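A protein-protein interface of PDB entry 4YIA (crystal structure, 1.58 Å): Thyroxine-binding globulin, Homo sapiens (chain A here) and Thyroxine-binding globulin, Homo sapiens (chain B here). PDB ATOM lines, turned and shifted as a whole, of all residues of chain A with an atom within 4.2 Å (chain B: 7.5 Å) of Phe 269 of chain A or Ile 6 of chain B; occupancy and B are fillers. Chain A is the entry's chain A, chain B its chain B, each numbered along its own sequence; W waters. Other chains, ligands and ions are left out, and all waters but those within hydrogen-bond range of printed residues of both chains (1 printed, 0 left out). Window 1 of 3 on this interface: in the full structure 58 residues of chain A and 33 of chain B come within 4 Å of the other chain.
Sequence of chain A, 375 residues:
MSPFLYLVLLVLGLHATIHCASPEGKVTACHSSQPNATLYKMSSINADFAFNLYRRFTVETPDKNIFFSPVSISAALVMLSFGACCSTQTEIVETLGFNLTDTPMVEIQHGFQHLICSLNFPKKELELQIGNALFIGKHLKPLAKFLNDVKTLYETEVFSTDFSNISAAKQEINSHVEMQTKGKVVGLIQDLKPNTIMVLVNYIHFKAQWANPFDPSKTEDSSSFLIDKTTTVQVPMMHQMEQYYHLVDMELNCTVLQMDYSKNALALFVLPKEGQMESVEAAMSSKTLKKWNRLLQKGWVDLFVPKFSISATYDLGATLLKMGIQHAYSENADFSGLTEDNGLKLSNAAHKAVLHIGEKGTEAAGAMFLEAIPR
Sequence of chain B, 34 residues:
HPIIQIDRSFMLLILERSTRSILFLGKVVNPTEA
O of Met 11 of chain B lies within hydrogen-bond range of N of Val 270 of chain A, at 2.9 Å. N of Phe 304 of chain A is in hydrogen-bond range of O of Ile 4 of chain B (3.0 Å). The backbone NH of Ile 6 of chain B is in hydrogen-bond range of the backbone carbonyl oxygen of Phe 304 of chain A (2.9 Å). The backbone NH (N) of Leu 268 of chain A is in hydrogen-bond range of the backbone carbonyl oxygen (O) of Leu 13 of chain B, at 2.9 Å.
The side-chain sulfur of Met 237 of chain A sits close to the backbone NH of Val 305 of chain A, at 3.7 Å. The backbone NH (N) of Leu 271 of chain A sits at hydrogen-bond distance from the backbone carbonyl oxygen (O) of Thr 255 of chain A (2.8 Å). The backbone NH (N) of Phe 269 of chain A lies within hydrogen-bond range of the backbone carbonyl oxygen (O) of Leu 257 of chain A, at 2.8 Å. O of Phe 10 of chain B is in hydrogen-bond range of N of Val 28 of chain B (2.9 Å). The guanidinium group (NH1) of Arg 8 of chain B lies within salt-bridge range of the side-chain carboxylate (OD1) of Asp 7 of chain B.
Asp 7 of chain B touches Met 237 of chain A (CB to CE, 3.97 Å). Thr 255 of chain A touches Ile 4 of chain B (CG2 to CD1, 3.7 Å). CA of Ala 267 of chain A touches O of Leu 13 of chain B (3.3 Å). O of Leu 268 of chain A touches O of Met 11 of chain B (3.9 Å). Phe 269 of chain A touches Met 11 of chain B. Leu 271 of chain A touches Arg 8 of chain B (CG to NH2, 3.8 Å). Leu 271 of chain A touches Ser 9 of chain B (CD1 to O, 3.8 Å). Phe 304 of chain A touches Ile 3 of chain B. Phe 304 of chain A touches Gln 5 of chain B. CD of Pro 306 of chain A touches O of Ile 6 of chain B, at 3.3 Å.
Phe 269 of chain A touches four residues of chain B. Ile 6 of chain B touches just these residues of chain A: Phe 225 (3.7 Å), Met 237 (3.6 Å), Phe 269 (3.9 Å), Phe 304 (2.9 Å) and Pro 306 (3.3 Å). Of the printed residues of chain A, Phe 10 of chain B touches Phe 225, Phe 269 and Val 270. Printed residues of chain A within 4 Å of Asp 7 of chain B: Phe 225 (3.4 Å) and Met 237 (3.97 Å). The nearest residue of chain B that does not touch Phe 269 of chain A is Leu 13 of chain B (5.2 Å). The nearest residue of chain A that does not touch Ile 6 of chain B is Val 305 of chain A (4.1 Å).
Of the 13 printed residues of chain B, 12 touch a printed residue of chain A. Hydrophobic or aromatic side chains of chain B within 4 Å of the printed part of chain A: Ile 3, Ile 4, Ile 6, Phe 10, Met 11, Leu 12, Leu 13 and Pro 31. Printed residues of chain A that touch a printed residue of chain B: Phe 225, Met 237, Thr 255, Ala 267, Leu 268, Phe 269, Val 270, Leu 271, Phe 304 and Pro 306. Along chain A the printed residues that touch a printed residue of chain B span positions 225 to 306. Among the printed residues, 26 pairs touch across the chains. Among the printed residues, no Asp or Glu carboxylate lies within 4 Å of a Lys or Arg side-chain nitrogen of the other chain.
Water W1 lies within hydrogen-bond range of the backbone carbonyl oxygen (O) of Leu 271 of chain A, the guanidinium group (NH2) of Arg 8 of chain B and the side-chain hydroxyl (OG1) of Thr 255 of chain A.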
ATOM      1  N   PHE A 225      14.271  25.316  18.424  1.00  0.00           N
ATOM      2  CA  PHE A 225      14.681  26.023  19.667  1.00  0.00           C
ATOM      3  C   PHE A 225      15.532  27.188  19.193  1.00  0.00           C
ATOM      4  O   PHE A 225      16.513  26.983  18.447  1.00  0.00           O
ATOM      5  CB  PHE A 225      15.459  25.112  20.490  1.00  0.00           C
ATOM      6  CG  PHE A 225      15.847  25.689  21.851  1.00  0.00           C
ATOM      7  CD1 PHE A 225      16.934  26.544  22.005  1.00  0.00           C
ATOM      8  CD2 PHE A 225      15.115  25.364  22.982  1.00  0.00           C
ATOM      9  CE1 PHE A 225      17.297  27.065  23.239  1.00  0.00           C
ATOM     10  CE2 PHE A 225      15.465  25.865  24.200  1.00  0.00           C
ATOM     11  CZ  PHE A 225      16.542  26.735  24.352  1.00  0.00           C
ATOM     12  N   MET A 237      10.955  18.012  21.709  1.00  0.00           N
ATOM     13  CA  MET A 237      10.185  18.905  22.580  1.00  0.00           C
ATOM     14  C   MET A 237       9.130  18.078  23.281  1.00  0.00           C
ATOM     15  O   MET A 237       8.186  17.632  22.664  1.00  0.00           O
ATOM     16  CB  MET A 237       9.628  20.116  21.806  1.00  0.00           C
ATOM     17  CG  MET A 237       8.981  21.142  22.638  1.00  0.00           C
ATOM     18  SD  MET A 237      10.236  22.072  23.568  1.00  0.00           S
ATOM     19  CE  MET A 237      10.960  23.174  22.401  1.00  0.00           C
ATOM     20  N   THR A 255       9.028  34.633  32.652  1.00  0.00           N
ATOM     21  CA  THR A 255       8.191  33.548  33.117  1.00  0.00           C
ATOM     22  C   THR A 255       8.986  32.596  33.972  1.00  0.00           C
ATOM     23  O   THR A 255      10.084  32.254  33.628  1.00  0.00           O
ATOM     24  CB  THR A 255       7.529  32.852  31.912  1.00  0.00           C
ATOM     25  OG1 THR A 255       6.653  33.803  31.233  1.00  0.00           O
ATOM     26  CG2 THR A 255       6.795  31.604  32.338  1.00  0.00           C
ATOM     27  N   VAL A 256       8.402  32.167  35.128  1.00  0.00           N
ATOM     28  CA  VAL A 256       9.036  31.180  36.017  1.00  0.00           C
ATOM     29  C   VAL A 256       8.099  29.999  36.143  1.00  0.00           C
ATOM     30  O   VAL A 256       6.916  30.166  36.384  1.00  0.00           O
ATOM     31  CB  VAL A 256       9.304  31.832  37.419  1.00  0.00           C
ATOM     32  CG1 VAL A 256      10.039  30.880  38.362  1.00  0.00           C
ATOM     33  CG2 VAL A 256      10.066  33.130  37.266  1.00  0.00           C
ATOM     34  N   LEU A 257       8.626  28.764  35.950  1.00  0.00           N
ATOM     35  CA  LEU A 257       7.866  27.536  35.944  1.00  0.00           C
ATOM     36  C   LEU A 257       8.582  26.556  36.821  1.00  0.00           C
ATOM     37  O   LEU A 257       9.817  26.356  36.730  1.00  0.00           O
ATOM     38  CB  LEU A 257       7.767  27.043  34.531  1.00  0.00           C
ATOM     39  CG  LEU A 257       7.015  25.805  34.055  1.00  0.00           C
ATOM     40  CD1 LEU A 257       7.721  24.602  34.365  1.00  0.00           C
ATOM     41  CD2 LEU A 257       5.620  25.685  34.511  1.00  0.00           C
ATOM     42  N   ALA A 267      12.788  21.639  40.182  1.00  0.00           N
ATOM     43  CA  ALA A 267      13.450  22.388  39.151  1.00  0.00           C
ATOM     44  C   ALA A 267      12.695  23.736  38.967  1.00  0.00           C
ATOM     45  O   ALA A 267      11.457  23.749  38.901  1.00  0.00           O
ATOM     46  CB  ALA A 267      13.532  21.624  37.848  1.00  0.00           C
ATOM     47  N   LEU A 268      13.453  24.824  38.738  1.00  0.00           N
ATOM     48  CA  LEU A 268      12.916  26.071  38.303  1.00  0.00           C
ATOM     49  C   LEU A 268      13.430  26.415  36.914  1.00  0.00           C
ATOM     50  O   LEU A 268      14.650  26.391  36.731  1.00  0.00           O
ATOM     51  CB  LEU A 268      13.298  27.177  39.256  1.00  0.00           C
ATOM     52  CG  LEU A 268      12.695  27.158  40.667  1.00  0.00           C
ATOM     53  CD1 LEU A 268      13.149  28.453  41.327  1.00  0.00           C
ATOM     54  CD2 LEU A 268      11.172  27.149  40.600  1.00  0.00           C
ATOM     55  N   PHE A 269      12.521  26.735  36.023  1.00  0.00           N
ATOM     56  CA  PHE A 269      12.856  27.180  34.646  1.00  0.00           C
ATOM     57  C   PHE A 269      12.493  28.665  34.527  1.00  0.00           C
ATOM     58  O   PHE A 269      11.394  29.064  34.960  1.00  0.00           O
ATOM     59  CB  PHE A 269      12.041  26.405  33.602  1.00  0.00           C
ATOM     60  CG  PHE A 269      12.412  24.910  33.460  1.00  0.00           C
ATOM     61  CD1 PHE A 269      11.939  24.045  34.402  1.00  0.00           C
ATOM     62  CD2 PHE A 269      13.220  24.489  32.474  1.00  0.00           C
ATOM     63  CE1 PHE A 269      12.238  22.696  34.326  1.00  0.00           C
ATOM     64  CE2 PHE A 269      13.495  23.105  32.385  1.00  0.00           C
ATOM     65  CZ  PHE A 269      13.021  22.301  33.283  1.00  0.00           C
ATOM     66  N   VAL A 270      13.452  29.472  34.119  1.00  0.00           N
ATOM     67  CA  VAL A 270      13.314  30.968  34.121  1.00  0.00           C
ATOM     68  C   VAL A 270      13.474  31.360  32.617  1.00  0.00           C
ATOM     69  O   VAL A 270      14.525  31.173  32.029  1.00  0.00           O
ATOM     70  CB  VAL A 270      14.388  31.570  34.923  1.00  0.00           C
ATOM     71  CG1 VAL A 270      14.205  33.094  34.899  1.00  0.00           C
ATOM     72  CG2 VAL A 270      14.267  31.197  36.371  1.00  0.00           C
ATOM     73  N   LEU A 271      12.387  31.825  32.009  1.00  0.00           N
ATOM     74  CA  LEU A 271      12.300  32.134  30.580  1.00  0.00           C
ATOM     75  C   LEU A 271      12.117  33.653  30.410  1.00  0.00           C
ATOM     76  O   LEU A 271      10.986  34.130  30.544  1.00  0.00           O
ATOM     77  CB  LEU A 271      11.141  31.300  29.952  1.00  0.00           C
ATOM     78  CG  LEU A 271      10.993  31.461  28.449  1.00  0.00           C
ATOM     79  CD1 LEU A 271      12.132  30.747  27.759  1.00  0.00           C
ATOM     80  CD2 LEU A 271       9.645  30.923  27.986  1.00  0.00           C
ATOM     81  N   PHE A 304       5.636  23.066  27.072  1.00  0.00           N
ATOM     82  CA  PHE A 304       6.598  22.475  26.139  1.00  0.00           C
ATOM     83  C   PHE A 304       7.995  22.657  26.717  1.00  0.00           C
ATOM     84  O   PHE A 304       8.397  23.771  26.936  1.00  0.00           O
ATOM     85  CB  PHE A 304       6.481  23.113  24.785  1.00  0.00           C
ATOM     86  CG  PHE A 304       5.104  22.970  24.123  1.00  0.00           C
ATOM     87  CD1 PHE A 304       4.053  23.833  24.479  1.00  0.00           C
ATOM     88  CD2 PHE A 304       4.917  22.015  23.138  1.00  0.00           C
ATOM     89  CE1 PHE A 304       2.799  23.696  23.914  1.00  0.00           C
ATOM     90  CE2 PHE A 304       3.641  21.871  22.553  1.00  0.00           C
ATOM     91  CZ  PHE A 304       2.645  22.757  22.938  1.00  0.00           C
ATOM     92  N   VAL A 305       8.739  21.603  26.879  1.00  0.00           N
ATOM     93  CA  VAL A 305      10.110  21.562  27.534  1.00  0.00           C
ATOM     94  C   VAL A 305      11.017  20.705  26.633  1.00  0.00           C
ATOM     95  O   VAL A 305      10.657  19.571  26.350  1.00  0.00           O
ATOM     96  CB  VAL A 305      10.051  20.887  28.963  1.00  0.00           C
ATOM     97  CG1 VAL A 305      11.526  20.826  29.558  1.00  0.00           C
ATOM     98  CG2 VAL A 305       9.189  21.680  29.918  1.00  0.00           C
ATOM     99  N   PRO A 306      12.235  21.151  26.316  1.00  0.00           N
ATOM    100  CA  PRO A 306      13.154  20.254  25.500  1.00  0.00           C
ATOM    101  C   PRO A 306      13.713  19.125  26.287  1.00  0.00           C
ATOM    102  O   PRO A 306      13.934  19.217  27.508  1.00  0.00           O
ATOM    103  CB  PRO A 306      14.263  21.204  25.061  1.00  0.00           C
ATOM    104  CG  PRO A 306      14.197  22.331  26.077  1.00  0.00           C
ATOM    105  CD  PRO A 306      12.788  22.504  26.482  1.00  0.00           C
ATOM    106  N   ILE B   3      -0.100  28.950  27.639  1.00  0.00           N
ATOM    107  CA  ILE B   3       1.003  28.140  27.064  1.00  0.00           C
ATOM    108  C   ILE B   3       2.333  28.669  27.627  1.00  0.00           C
ATOM    109  O   ILE B   3       2.595  29.931  27.623  1.00  0.00           O
ATOM    110  CB  ILE B   3       0.985  28.196  25.532  1.00  0.00           C
ATOM    111  CG1 ILE B   3      -0.356  27.651  25.031  1.00  0.00           C
ATOM    112  CG2 ILE B   3       2.148  27.495  24.908  1.00  0.00           C
ATOM    113  CD1 ILE B   3      -0.993  28.504  23.944  1.00  0.00           C
ATOM    114  N   ILE B   4       3.209  27.761  27.986  1.00  0.00           N
ATOM    115  CA  ILE B   4       4.628  28.098  28.338  1.00  0.00           C
ATOM    116  C   ILE B   4       5.453  27.253  27.411  1.00  0.00           C
ATOM    117  O   ILE B   4       5.370  25.979  27.499  1.00  0.00           O
ATOM    118  CB  ILE B   4       4.990  27.965  29.803  1.00  0.00           C
ATOM    119  CG1 ILE B   4       4.208  28.988  30.694  1.00  0.00           C
ATOM    120  CG2 ILE B   4       6.485  28.178  30.016  1.00  0.00           C
ATOM    121  CD1 ILE B   4       4.367  28.835  32.198  1.00  0.00           C
ATOM    122  N   GLN B   5       6.132  27.895  26.454  1.00  0.00           N
ATOM    123  CA  GLN B   5       6.958  27.123  25.473  1.00  0.00           C
ATOM    124  C   GLN B   5       8.456  27.469  25.717  1.00  0.00           C
ATOM    125  O   GLN B   5       8.850  28.645  25.444  1.00  0.00           O
ATOM    126  CB  GLN B   5       6.624  27.469  24.045  1.00  0.00           C
ATOM    127  CG  GLN B   5       5.399  26.817  23.535  1.00  0.00           C
ATOM    128  CD  GLN B   5       5.250  27.134  22.044  1.00  0.00           C
ATOM    129  OE1 GLN B   5       5.579  26.302  21.174  1.00  0.00           O
ATOM    130  NE2 GLN B   5       4.929  28.333  21.765  1.00  0.00           N
ATOM    131  N   ILE B   6       9.198  26.507  26.200  1.00  0.00           N
ATOM    132  CA  ILE B   6      10.612  26.718  26.578  1.00  0.00           C
ATOM    133  C   ILE B   6      11.381  26.412  25.270  1.00  0.00           C
ATOM    134  O   ILE B   6      11.912  25.315  25.086  1.00  0.00           O
ATOM    135  CB  ILE B   6      11.055  25.878  27.757  1.00  0.00           C
ATOM    136  CG1 ILE B   6      10.106  26.311  28.900  1.00  0.00           C
ATOM    137  CG2 ILE B   6      12.563  26.113  28.059  1.00  0.00           C
ATOM    138  CD1 ILE B   6      10.296  25.652  30.202  1.00  0.00           C
ATOM    139  N   ASP B   7      11.357  27.359  24.378  1.00  0.00           N
ATOM    140  CA  ASP B   7      11.921  27.217  23.041  1.00  0.00           C
ATOM    141  C   ASP B   7      12.888  28.289  22.666  1.00  0.00           C
ATOM    142  O   ASP B   7      13.150  28.481  21.455  1.00  0.00           O
ATOM    143  CB  ASP B   7      10.782  27.126  22.039  1.00  0.00           C
ATOM    144  CG  ASP B   7      10.056  28.404  21.840  1.00  0.00           C
ATOM    145  OD1 ASP B   7      10.204  29.400  22.570  1.00  0.00           O
ATOM    146  OD2 ASP B   7       9.163  28.336  20.922  1.00  0.00           O
ATOM    147  N   ARG B   8      13.505  28.885  23.671  1.00  0.00           N
ATOM    148  CA  ARG B   8      14.584  29.860  23.543  1.00  0.00           C
ATOM    149  C   ARG B   8      15.407  29.869  24.831  1.00  0.00           C
ATOM    150  O   ARG B   8      15.017  29.196  25.804  1.00  0.00           O
ATOM    151  CB  ARG B   8      13.998  31.220  23.162  1.00  0.00           C
ATOM    152  CG  ARG B   8      13.158  31.937  24.149  1.00  0.00           C
ATOM    153  CD  ARG B   8      12.881  33.417  23.740  1.00  0.00           C
ATOM    154  NE  ARG B   8      12.085  33.978  24.827  1.00  0.00           N
ATOM    155  CZ  ARG B   8      10.796  33.705  24.974  1.00  0.00           C
ATOM    156  NH1 ARG B   8      10.130  33.002  24.036  1.00  0.00           N
ATOM    157  NH2 ARG B   8      10.132  34.192  25.993  1.00  0.00           N
ATOM    158  N   SER B   9      16.432  30.723  24.914  1.00  0.00           N
ATOM    159  CA  SER B   9      17.364  30.575  26.036  1.00  0.00           C
ATOM    160  C   SER B   9      16.653  30.713  27.382  1.00  0.00           C
ATOM    161  O   SER B   9      15.796  31.593  27.562  1.00  0.00           O
ATOM    162  CB  SER B   9      18.401  31.674  26.020  1.00  0.00           C
ATOM    163  OG  SER B   9      19.214  31.568  24.876  1.00  0.00           O
ATOM    164  N   PHE B  10      17.043  29.867  28.314  1.00  0.00           N
ATOM    165  CA  PHE B  10      16.438  29.874  29.672  1.00  0.00           C
ATOM    166  C   PHE B  10      17.494  29.619  30.715  1.00  0.00           C
ATOM    167  O   PHE B  10      18.479  28.982  30.441  1.00  0.00           O
ATOM    168  CB  PHE B  10      15.266  28.838  29.697  1.00  0.00           C
ATOM    169  CG  PHE B  10      15.637  27.401  29.535  1.00  0.00           C
ATOM    170  CD1 PHE B  10      15.788  26.851  28.271  1.00  0.00           C
ATOM    171  CD2 PHE B  10      15.834  26.562  30.649  1.00  0.00           C
ATOM    172  CE1 PHE B  10      16.023  25.493  28.085  1.00  0.00           C
ATOM    173  CE2 PHE B  10      16.138  25.237  30.509  1.00  0.00           C
ATOM    174  CZ  PHE B  10      16.275  24.695  29.201  1.00  0.00           C
ATOM    175  N   MET B  11      17.224  30.006  31.950  1.00  0.00           N
ATOM    176  CA  MET B  11      18.040  29.627  33.118  1.00  0.00           C
ATOM    177  C   MET B  11      17.299  28.481  33.803  1.00  0.00           C
ATOM    178  O   MET B  11      16.063  28.357  33.726  1.00  0.00           O
ATOM    179  CB  MET B  11      18.211  30.802  34.070  1.00  0.00           C
ATOM    180  CG  MET B  11      19.320  31.732  33.618  1.00  0.00           C
ATOM    181  SD  MET B  11      19.540  33.159  34.727  1.00  0.00           S
ATOM    182  CE  MET B  11      20.592  32.395  35.902  1.00  0.00           C
ATOM    183  N   LEU B  12      18.068  27.590  34.454  1.00  0.00           N
ATOM    184  CA  LEU B  12      17.602  26.434  35.150  1.00  0.00           C
ATOM    185  C   LEU B  12      18.219  26.387  36.549  1.00  0.00           C
ATOM    186  O   LEU B  12      19.444  26.613  36.689  1.00  0.00           O
ATOM    187  CB  LEU B  12      18.055  25.217  34.413  1.00  0.00           C
ATOM    188  CG  LEU B  12      17.712  23.880  34.965  1.00  0.00           C
ATOM    189  CD1 LEU B  12      16.194  23.593  35.048  1.00  0.00           C
ATOM    190  CD2 LEU B  12      18.351  22.620  34.371  1.00  0.00           C
ATOM    191  N   LEU B  13      17.419  26.087  37.569  1.00  0.00           N
ATOM    192  CA  LEU B  13      17.912  25.827  38.919  1.00  0.00           C
ATOM    193  C   LEU B  13      17.365  24.470  39.357  1.00  0.00           C
ATOM    194  O   LEU B  13      16.227  24.127  39.045  1.00  0.00           O
ATOM    195  CB  LEU B  13      17.416  26.880  39.898  1.00  0.00           C
ATOM    196  CG  LEU B  13      17.822  28.327  39.625  1.00  0.00           C
ATOM    197  CD1 LEU B  13      16.831  29.016  38.725  1.00  0.00           C
ATOM    198  CD2 LEU B  13      17.877  28.943  41.016  1.00  0.00           C
ATOM    199  N   VAL B  28      20.743  27.565  29.420  1.00  0.00           N
ATOM    200  CA  VAL B  28      20.760  26.788  28.228  1.00  0.00           C
ATOM    201  C   VAL B  28      20.534  27.775  27.094  1.00  0.00           C
ATOM    202  O   VAL B  28      19.426  28.317  26.958  1.00  0.00           O
ATOM    203  CB  VAL B  28      19.685  25.712  28.248  1.00  0.00           C
ATOM    204  CG1 VAL B  28      19.733  24.946  26.950  1.00  0.00           C
ATOM    205  CG2 VAL B  28      19.899  24.724  29.366  1.00  0.00           C
ATOM    206  N   PRO B  31      20.747  23.807  23.281  1.00  0.00           N
ATOM    207  CA  PRO B  31      20.591  22.486  23.940  1.00  0.00           C
ATOM    208  C   PRO B  31      21.253  21.331  23.184  1.00  0.00           C
ATOM    209  O   PRO B  31      21.300  20.206  23.749  1.00  0.00           O
ATOM    210  CB  PRO B  31      19.098  22.321  24.022  1.00  0.00           C
ATOM    211  CG  PRO B  31      18.521  23.279  23.036  1.00  0.00           C
ATOM    212  CD  PRO B  31      19.430  24.384  22.899  1.00  0.00           C
HETATM  213  O   HOH W   1       8.874  34.800  28.878  1.00  0.00           O
